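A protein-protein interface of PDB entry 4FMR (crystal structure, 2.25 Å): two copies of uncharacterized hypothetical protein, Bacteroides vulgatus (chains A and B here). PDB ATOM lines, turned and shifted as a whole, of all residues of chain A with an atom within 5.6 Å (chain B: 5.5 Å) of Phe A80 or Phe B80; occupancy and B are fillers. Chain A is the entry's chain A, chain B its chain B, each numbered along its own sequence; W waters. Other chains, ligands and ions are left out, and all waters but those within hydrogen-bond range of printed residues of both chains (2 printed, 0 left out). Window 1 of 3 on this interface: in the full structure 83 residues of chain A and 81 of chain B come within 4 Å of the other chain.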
ATOM      1  N   VAL A  65     -15.799 -27.041 -26.428  1.00  0.00           N
ATOM      2  CA  VAL A  65     -16.171 -26.811 -25.030  1.00  0.00           C
ATOM      3  C   VAL A  65     -16.436 -25.311 -24.787  1.00  0.00           C
ATOM      4  O   VAL A  65     -17.468 -24.992 -24.193  1.00  0.00           O
ATOM      5  CB  VAL A  65     -15.130 -27.387 -24.048  1.00  0.00           C
ATOM      6  CG1 VAL A  65     -15.411 -26.947 -22.606  1.00  0.00           C
ATOM      7  CG2 VAL A  65     -15.104 -28.914 -24.140  1.00  0.00           C
ATOM      8  N   LEU A  69     -20.105 -23.799 -23.591  1.00  0.00           N
ATOM      9  CA  LEU A  69     -20.254 -22.983 -22.393  1.00  0.00           C
ATOM     10  C   LEU A  69     -20.796 -21.594 -22.701  1.00  0.00           C
ATOM     11  O   LEU A  69     -21.628 -21.077 -21.940  1.00  0.00           O
ATOM     12  CB  LEU A  69     -18.885 -22.868 -21.667  1.00  0.00           C
ATOM     13  CG  LEU A  69     -18.403 -24.175 -21.033  1.00  0.00           C
ATOM     14  CD1 LEU A  69     -16.921 -24.118 -20.686  1.00  0.00           C
ATOM     15  CD2 LEU A  69     -19.247 -24.527 -19.818  1.00  0.00           C
ATOM     16  N   VAL A  75     -21.007 -28.338 -19.183  1.00  0.00           N
ATOM     17  CA  VAL A  75     -20.139 -29.298 -19.848  1.00  0.00           C
ATOM     18  C   VAL A  75     -19.505 -30.213 -18.831  1.00  0.00           C
ATOM     19  O   VAL A  75     -18.853 -29.731 -17.910  1.00  0.00           O
ATOM     20  CB  VAL A  75     -19.065 -28.581 -20.701  1.00  0.00           C
ATOM     21  CG1 VAL A  75     -18.070 -29.582 -21.304  1.00  0.00           C
ATOM     22  CG2 VAL A  75     -19.719 -27.730 -21.789  1.00  0.00           C
ATOM     23  N   ASN A  76     -19.624 -31.520 -19.035  1.00  0.00           N
ATOM     24  CA  ASN A  76     -19.005 -32.471 -18.122  1.00  0.00           C
ATOM     25  C   ASN A  76     -17.995 -33.370 -18.870  1.00  0.00           C
ATOM     26  O   ASN A  76     -18.367 -34.133 -19.763  1.00  0.00           O
ATOM     27  CB  ASN A  76     -20.102 -33.328 -17.410  1.00  0.00           C
ATOM     28  CG  ASN A  76     -19.580 -34.471 -16.553  1.00  0.00           C
ATOM     29  OD1 ASN A  76     -18.485 -34.409 -15.977  1.00  0.00           O
ATOM     30  ND2 ASN A  76     -20.351 -35.553 -16.447  1.00  0.00           N
ATOM     31  N   THR A  77     -16.714 -33.306 -18.463  1.00  0.00           N
ATOM     32  CA  THR A  77     -15.650 -34.205 -18.964  1.00  0.00           C
ATOM     33  C   THR A  77     -15.256 -35.119 -17.782  1.00  0.00           C
ATOM     34  O   THR A  77     -15.828 -35.025 -16.696  1.00  0.00           O
ATOM     35  CB  THR A  77     -14.455 -33.386 -19.536  1.00  0.00           C
ATOM     36  OG1 THR A  77     -13.717 -32.789 -18.457  1.00  0.00           O
ATOM     37  CG2 THR A  77     -14.892 -32.298 -20.526  1.00  0.00           C
ATOM     38  N   GLY A  78     -14.240 -35.938 -17.955  1.00  0.00           N
ATOM     39  CA  GLY A  78     -13.748 -36.737 -16.843  1.00  0.00           C
ATOM     40  C   GLY A  78     -13.045 -35.856 -15.833  1.00  0.00           C
ATOM     41  O   GLY A  78     -13.128 -36.115 -14.626  1.00  0.00           O
ATOM     42  N   LEU A  79     -12.393 -34.757 -16.318  1.00  0.00           N
ATOM     43  CA  LEU A  79     -11.627 -33.837 -15.476  1.00  0.00           C
ATOM     44  C   LEU A  79     -12.472 -32.792 -14.768  1.00  0.00           C
ATOM     45  O   LEU A  79     -12.130 -32.396 -13.648  1.00  0.00           O
ATOM     46  CB  LEU A  79     -10.561 -33.089 -16.307  1.00  0.00           C
ATOM     47  CG  LEU A  79      -9.404 -33.898 -16.851  1.00  0.00           C
ATOM     48  CD1 LEU A  79      -8.473 -32.997 -17.638  1.00  0.00           C
ATOM     49  CD2 LEU A  79      -8.628 -34.642 -15.708  1.00  0.00           C
ATOM     50  N   PHE A  80     -13.497 -32.257 -15.435  1.00  0.00           N
ATOM     51  CA  PHE A  80     -14.254 -31.183 -14.812  1.00  0.00           C
ATOM     52  C   PHE A  80     -15.681 -31.095 -15.306  1.00  0.00           C
ATOM     53  O   PHE A  80     -16.063 -31.680 -16.314  1.00  0.00           O
ATOM     54  CB  PHE A  80     -13.562 -29.820 -15.081  1.00  0.00           C
ATOM     55  CG  PHE A  80     -13.502 -29.424 -16.545  1.00  0.00           C
ATOM     56  CD1 PHE A  80     -14.593 -28.812 -17.167  1.00  0.00           C
ATOM     57  CD2 PHE A  80     -12.356 -29.656 -17.298  1.00  0.00           C
ATOM     58  CE1 PHE A  80     -14.554 -28.488 -18.530  1.00  0.00           C
ATOM     59  CE2 PHE A  80     -12.303 -29.307 -18.656  1.00  0.00           C
ATOM     60  CZ  PHE A  80     -13.406 -28.740 -19.268  1.00  0.00           C
ATOM     61  N   ARG A  81     -16.441 -30.297 -14.603  1.00  0.00           N
ATOM     62  CA  ARG A  81     -17.768 -29.867 -15.012  1.00  0.00           C
ATOM     63  C   ARG A  81     -17.717 -28.351 -14.982  1.00  0.00           C
ATOM     64  O   ARG A  81     -17.174 -27.775 -14.030  1.00  0.00           O
ATOM     65  CB  ARG A  81     -18.906 -30.476 -14.158  1.00  0.00           C
ATOM     66  CG  ARG A  81     -20.296 -30.012 -14.564  1.00  0.00           C
ATOM     67  CD  ARG A  81     -20.663 -28.729 -13.842  1.00  0.00           C
ATOM     68  NE  ARG A  81     -22.093 -28.471 -13.938  1.00  0.00           N
ATOM     69  CZ  ARG A  81     -22.712 -27.495 -13.302  1.00  0.00           C
ATOM     70  NH1 ARG A  81     -22.034 -26.676 -12.506  1.00  0.00           N
ATOM     71  NH2 ARG A  81     -24.021 -27.354 -13.417  1.00  0.00           N
ATOM     72  N   GLY A  82     -18.181 -27.728 -16.057  1.00  0.00           N
ATOM     73  CA  GLY A  82     -18.217 -26.276 -16.174  1.00  0.00           C
ATOM     74  C   GLY A  82     -19.579 -25.748 -16.574  1.00  0.00           C
ATOM     75  O   GLY A  82     -20.347 -26.442 -17.238  1.00  0.00           O
ATOM     76  N   LEU A 106     -15.906 -23.838 -12.685  1.00  0.00           N
ATOM     77  CA  LEU A 106     -15.425 -25.196 -12.890  1.00  0.00           C
ATOM     78  C   LEU A 106     -15.303 -25.952 -11.599  1.00  0.00           C
ATOM     79  O   LEU A 106     -14.827 -25.417 -10.596  1.00  0.00           O
ATOM     80  CB  LEU A 106     -14.051 -25.182 -13.585  1.00  0.00           C
ATOM     81  CG  LEU A 106     -13.948 -24.464 -14.926  1.00  0.00           C
ATOM     82  CD1 LEU A 106     -12.524 -24.146 -15.229  1.00  0.00           C
ATOM     83  CD2 LEU A 106     -14.545 -25.301 -16.047  1.00  0.00           C
ATOM     84  N   THR A 107     -15.736 -27.210 -11.627  1.00  0.00           N
ATOM     85  CA  THR A 107     -15.668 -28.071 -10.462  1.00  0.00           C
ATOM     86  C   THR A 107     -14.935 -29.341 -10.892  1.00  0.00           C
ATOM     87  O   THR A 107     -14.994 -29.695 -12.052  1.00  0.00           O
ATOM     88  CB  THR A 107     -17.060 -28.312  -9.839  1.00  0.00           C
ATOM     89  OG1 THR A 107     -16.867 -28.975  -8.594  1.00  0.00           O
ATOM     90  CG2 THR A 107     -18.000 -29.167 -10.735  1.00  0.00           C
ATOM     91  N   GLN A 108     -14.229 -30.007  -9.971  1.00  0.00           N
ATOM     92  CA  GLN A 108     -13.494 -31.226 -10.311  1.00  0.00           C
ATOM     93  C   GLN A 108     -14.476 -32.337 -10.808  1.00  0.00           C
ATOM     94  O   GLN A 108     -15.616 -32.455 -10.340  1.00  0.00           O
ATOM     95  CB  GLN A 108     -12.644 -31.708  -9.118  1.00  0.00           C
ATOM     96  CG  GLN A 108     -13.441 -32.388  -7.995  1.00  0.00           C
ATOM     97  CD  GLN A 108     -12.599 -32.735  -6.802  1.00  0.00           C
ATOM     98  OE1 GLN A 108     -11.512 -32.205  -6.610  1.00  0.00           O
ATOM     99  NE2 GLN A 108     -13.112 -33.595  -5.934  1.00  0.00           N
ATOM    100  N   GLY A 109     -14.006 -33.110 -11.783  1.00  0.00           N
ATOM    101  CA  GLY A 109     -14.782 -34.199 -12.356  1.00  0.00           C
ATOM    102  C   GLY A 109     -14.459 -35.545 -11.726  1.00  0.00           C
ATOM    103  O   GLY A 109     -13.564 -35.654 -10.872  1.00  0.00           O
ATOM    104  N   LEU A 112     -10.789 -36.794 -11.520  1.00  0.00           N
ATOM    105  CA  LEU A 112     -10.007 -36.170 -10.445  1.00  0.00           C
ATOM    106  C   LEU A 112     -10.408 -36.740  -9.067  1.00  0.00           C
ATOM    107  O   LEU A 112      -9.533 -37.065  -8.276  1.00  0.00           O
ATOM    108  CB  LEU A 112     -10.133 -34.647 -10.467  1.00  0.00           C
ATOM    109  CG  LEU A 112      -9.530 -33.974 -11.730  1.00  0.00           C
ATOM    110  CD1 LEU A 112      -9.662 -32.447 -11.643  1.00  0.00           C
ATOM    111  CD2 LEU A 112      -8.062 -34.413 -11.963  1.00  0.00           C
ATOM    112  N   VAL B  65      -2.967 -35.210 -16.965  1.00  0.00           N
ATOM    113  CA  VAL B  65      -3.411 -34.085 -16.149  1.00  0.00           C
ATOM    114  C   VAL B  65      -3.688 -34.583 -14.700  1.00  0.00           C
ATOM    115  O   VAL B  65      -3.208 -33.939 -13.757  1.00  0.00           O
ATOM    116  CB  VAL B  65      -4.640 -33.348 -16.774  1.00  0.00           C
ATOM    117  CG1 VAL B  65      -5.287 -32.392 -15.766  1.00  0.00           C
ATOM    118  CG2 VAL B  65      -4.236 -32.584 -18.041  1.00  0.00           C
ATOM    119  N   VAL B  75      -1.549 -27.266 -13.186  1.00  0.00           N
ATOM    120  CA  VAL B  75      -1.724 -27.638 -14.581  1.00  0.00           C
ATOM    121  C   VAL B  75      -2.540 -26.580 -15.288  1.00  0.00           C
ATOM    122  O   VAL B  75      -3.637 -26.247 -14.835  1.00  0.00           O
ATOM    123  CB  VAL B  75      -2.419 -29.041 -14.692  1.00  0.00           C
ATOM    124  CG1 VAL B  75      -2.695 -29.425 -16.170  1.00  0.00           C
ATOM    125  CG2 VAL B  75      -1.611 -30.127 -13.984  1.00  0.00           C
ATOM    126  N   ASN B  76      -2.053 -26.102 -16.426  1.00  0.00           N
ATOM    127  CA  ASN B  76      -2.758 -25.107 -17.224  1.00  0.00           C
ATOM    128  C   ASN B  76      -2.978 -25.604 -18.645  1.00  0.00           C
ATOM    129  O   ASN B  76      -2.019 -26.005 -19.292  1.00  0.00           O
ATOM    130  CB  ASN B  76      -1.956 -23.776 -17.249  1.00  0.00           C
ATOM    131  CG  ASN B  76      -2.500 -22.721 -18.193  1.00  0.00           C
ATOM    132  OD1 ASN B  76      -3.710 -22.445 -18.242  1.00  0.00           O
ATOM    133  ND2 ASN B  76      -1.613 -22.092 -18.957  1.00  0.00           N
ATOM    134  N   THR B  77      -4.218 -25.556 -19.138  1.00  0.00           N
ATOM    135  CA  THR B  77      -4.584 -25.845 -20.537  1.00  0.00           C
ATOM    136  C   THR B  77      -5.249 -24.541 -21.003  1.00  0.00           C
ATOM    137  O   THR B  77      -5.324 -23.592 -20.222  1.00  0.00           O
ATOM    138  CB  THR B  77      -5.458 -27.116 -20.652  1.00  0.00           C
ATOM    139  OG1 THR B  77      -6.760 -26.847 -20.126  1.00  0.00           O
ATOM    140  CG2 THR B  77      -4.846 -28.344 -19.960  1.00  0.00           C
ATOM    141  N   GLY B  78      -5.808 -24.494 -22.196  1.00  0.00           N
ATOM    142  CA  GLY B  78      -6.535 -23.301 -22.613  1.00  0.00           C
ATOM    143  C   GLY B  78      -7.881 -23.185 -21.912  1.00  0.00           C
ATOM    144  O   GLY B  78      -8.417 -22.085 -21.782  1.00  0.00           O
ATOM    145  N   LEU B  79      -8.430 -24.316 -21.424  1.00  0.00           N
ATOM    146  CA  LEU B  79      -9.730 -24.319 -20.767  1.00  0.00           C
ATOM    147  C   LEU B  79      -9.659 -24.033 -19.283  1.00  0.00           C
ATOM    148  O   LEU B  79     -10.628 -23.517 -18.742  1.00  0.00           O
ATOM    149  CB  LEU B  79     -10.441 -25.679 -20.956  1.00  0.00           C
ATOM    150  CG  LEU B  79     -10.950 -26.010 -22.359  1.00  0.00           C
ATOM    151  CD1 LEU B  79     -11.651 -27.328 -22.353  1.00  0.00           C
ATOM    152  CD2 LEU B  79     -11.894 -24.917 -22.900  1.00  0.00           C
ATOM    153  N   PHE B  80      -8.588 -24.420 -18.602  1.00  0.00           N
ATOM    154  CA  PHE B  80      -8.518 -24.243 -17.149  1.00  0.00           C
ATOM    155  C   PHE B  80      -7.105 -24.258 -16.604  1.00  0.00           C
ATOM    156  O   PHE B  80      -6.199 -24.802 -17.218  1.00  0.00           O
ATOM    157  CB  PHE B  80      -9.303 -25.381 -16.423  1.00  0.00           C
ATOM    158  CG  PHE B  80      -8.752 -26.778 -16.641  1.00  0.00           C
ATOM    159  CD1 PHE B  80      -7.679 -27.251 -15.883  1.00  0.00           C
ATOM    160  CD2 PHE B  80      -9.257 -27.591 -17.653  1.00  0.00           C
ATOM    161  CE1 PHE B  80      -7.089 -28.484 -16.166  1.00  0.00           C
ATOM    162  CE2 PHE B  80      -8.711 -28.858 -17.890  1.00  0.00           C
ATOM    163  CZ  PHE B  80      -7.621 -29.288 -17.155  1.00  0.00           C
ATOM    164  N   ARG B  81      -6.975 -23.776 -15.372  1.00  0.00           N
ATOM    165  CA  ARG B  81      -5.816 -23.942 -14.527  1.00  0.00           C
ATOM    166  C   ARG B  81      -6.288 -24.719 -13.286  1.00  0.00           C
ATOM    167  O   ARG B  81      -7.325 -24.396 -12.692  1.00  0.00           O
ATOM    168  CB  ARG B  81      -5.124 -22.626 -14.179  1.00  0.00           C
ATOM    169  CG  ARG B  81      -3.866 -22.797 -13.296  1.00  0.00           C
ATOM    170  CD  ARG B  81      -4.256 -22.737 -11.840  1.00  0.00           C
ATOM    171  NE  ARG B  81      -3.090 -22.500 -10.989  1.00  0.00           N
ATOM    172  CZ  ARG B  81      -3.170 -22.191  -9.707  1.00  0.00           C
ATOM    173  NH1 ARG B  81      -4.353 -22.093  -9.114  1.00  0.00           N
ATOM    174  NH2 ARG B  81      -2.072 -21.920  -9.016  1.00  0.00           N
ATOM    175  N   GLY B  82      -5.534 -25.755 -12.927  1.00  0.00           N
ATOM    176  CA  GLY B  82      -5.826 -26.577 -11.765  1.00  0.00           C
ATOM    177  C   GLY B  82      -4.628 -26.701 -10.853  1.00  0.00           C
ATOM    178  O   GLY B  82      -3.472 -26.646 -11.303  1.00  0.00           O
ATOM    179  N   LEU B 106     -10.255 -25.419  -9.591  1.00  0.00           N
ATOM    180  CA  LEU B 106     -10.163 -25.147 -11.010  1.00  0.00           C
ATOM    181  C   LEU B 106     -10.611 -23.743 -11.339  1.00  0.00           C
ATOM    182  O   LEU B 106     -11.589 -23.248 -10.790  1.00  0.00           O
ATOM    183  CB  LEU B 106     -10.978 -26.172 -11.824  1.00  0.00           C
ATOM    184  CG  LEU B 106     -10.527 -27.637 -11.703  1.00  0.00           C
ATOM    185  CD1 LEU B 106     -11.642 -28.540 -12.006  1.00  0.00           C
ATOM    186  CD2 LEU B 106      -9.314 -27.948 -12.608  1.00  0.00           C
ATOM    187  N   THR B 107      -9.864 -23.082 -12.230  1.00  0.00           N
ATOM    188  CA  THR B 107     -10.216 -21.735 -12.662  1.00  0.00           C
ATOM    189  C   THR B 107     -10.222 -21.726 -14.200  1.00  0.00           C
ATOM    190  O   THR B 107      -9.533 -22.543 -14.811  1.00  0.00           O
ATOM    191  CB  THR B 107      -9.311 -20.657 -12.030  1.00  0.00           C
ATOM    192  OG1 THR B 107      -9.888 -19.385 -12.324  1.00  0.00           O
ATOM    193  CG2 THR B 107      -7.873 -20.695 -12.543  1.00  0.00           C
ATOM    194  N   GLN B 108     -11.017 -20.833 -14.820  1.00  0.00           N
ATOM    195  CA  GLN B 108     -11.096 -20.753 -16.285  1.00  0.00           C
ATOM    196  C   GLN B 108      -9.721 -20.360 -16.900  1.00  0.00           C
ATOM    197  O   GLN B 108      -8.965 -19.570 -16.317  1.00  0.00           O
ATOM    198  CB  GLN B 108     -12.196 -19.763 -16.723  1.00  0.00           C
ATOM    199  CG  GLN B 108     -11.955 -18.299 -16.278  1.00  0.00           C
ATOM    200  CD  GLN B 108     -13.033 -17.340 -16.736  1.00  0.00           C
ATOM    201  OE1 GLN B 108     -14.226 -17.646 -16.725  1.00  0.00           O
ATOM    202  NE2 GLN B 108     -12.639 -16.134 -17.102  1.00  0.00           N
ATOM    203  N   GLY B 109      -9.407 -20.954 -18.042  1.00  0.00           N
ATOM    204  CA  GLY B 109      -8.174 -20.675 -18.765  1.00  0.00           C
ATOM    205  C   GLY B 109      -8.368 -19.617 -19.838  1.00  0.00           C
ATOM    206  O   GLY B 109      -9.459 -19.060 -19.992  1.00  0.00           O
ATOM    207  N   LEU B 112     -11.288 -19.837 -22.570  1.00  0.00           N
ATOM    208  CA  LEU B 112     -12.579 -19.431 -22.048  1.00  0.00           C
ATOM    209  C   LEU B 112     -12.648 -17.931 -21.899  1.00  0.00           C
ATOM    210  O   LEU B 112     -13.662 -17.348 -22.288  1.00  0.00           O
ATOM    211  CB  LEU B 112     -12.908 -20.131 -20.723  1.00  0.00           C
ATOM    212  CG  LEU B 112     -13.136 -21.655 -20.856  1.00  0.00           C
ATOM    213  CD1 LEU B 112     -13.491 -22.275 -19.509  1.00  0.00           C
ATOM    214  CD2 LEU B 112     -14.173 -21.976 -21.942  1.00  0.00           C
HETATM  215  O   HOH W   1     -13.053 -25.771  -8.543  1.00  0.00           O
HETATM  216  O   HOH W   2     -13.947 -21.948 -11.296  1.00  0.00           O
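O of Thr B107 lies within hydrogen-bond range of N of Arg B81.
The side-chain hydroxyl (OG1) of Thr A77 lies within hydrogen-bond range of the backbone NH (N) of Leu A79.
The backbone NH of Thr A107 is in hydrogen-bond range of the backbone carbonyl oxygen of Arg A81.
The backbone carbonyl oxygen of Leu A79 is in hydrogen-bond range of the backbone NH of Gly A109, at 2.7 Å.
The side-chain hydroxyl (OG1) of Thr B77 sits close to the backbone NH (N) of Leu B79 (3.3 Å).
O of Leu B79 lies within hydrogen-bond range of N of Gly B109, 2.9 Å away.
Among the printed residues, pairs that only touch across the chains: Val A65 with Leu B79 (3.8 Å), Leu A69 with Leu B112 (3.7 Å), Leu A79 with Val B65 (3.7 Å), Leu A79 with Phe B80 (3.8 Å), Phe A80 with Leu B79 (3.8 Å), Phe A80 with Phe B80 (3.6 Å), Phe A80 with Leu B106 (3.8 Å), Leu A106 with Phe B80 (3.7 Å), Leu A106 with Leu B106 (3.7 Å), Leu A106 with Thr B107 (3.4 Å), Leu A106 with Gln B108 (3.7 Å), Thr A107 with Leu B106 (3.5 Å) and Gln A108 with Leu B106 (3.6 Å).
Phe A80 touches three residues of chain B.
Of chain A, only Leu A79 (3.8 Å), Phe A80 (3.6 Å) and Leu A106 (3.7 Å) come within 4 Å of Phe B80.
Of the printed residues of chain B, Leu A69 touches Leu B112.
Of the printed residues of chain A, Leu B106 touches Phe A80 (3.8 Å), Leu A106 (3.7 Å), Thr A107 (3.5 Å) and Gln A108 (3.6 Å).
Printed residues of chain A within 4 Å of Gln B108: Leu A106 (3.7 Å).
The nearest printed residue of chain B that does not touch Phe A80 is Thr B77 (6.2 Å).
Of the 15 printed residues of chain A, 7 touch a printed residue of chain B.
Printed residues of chain A that touch a printed residue of chain B: Val A65, Leu A69, Leu A79, Phe A80, Leu A106, Thr A107 and Gln A108.
Of the 14 printed residues of chain B, 7 touch a printed residue of chain A.
Hydrophobic or aromatic side chains of chain B that line the printed part of chain A: Val B65, Leu B79, Phe B80, Leu B106 and Leu B112.
Among the printed residues, 13 pairs touch across the chains.
Val A65 touches Leu B79, and with the chains exchanged Leu A79 touches Val B65.
Phe A80 touches Leu B106, and with the chains exchanged Leu A106 touches Phe B80.
Leu A106 touches Thr B107, and with the chains exchanged Thr A107 touches Leu B106.
Leu A106 touches Gln B108, and with the chains exchanged Gln A108 touches Leu B106.
Positions printed for both chains: 65, 75, 76, 77, 78, 79, 80, 81, 82, 106, 107, 108, 109 and 112.
Of the 13 pairs that touch across the chains among the printed residues, 12 have their exchanged pair printed and touching as well.
Water W1 lies within hydrogen-bond range of O of Leu A106 (2.7 Å) and N of Leu B106 (3.0 Å).
Water W2 bridges O of Leu B106 and N of Leu A106.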
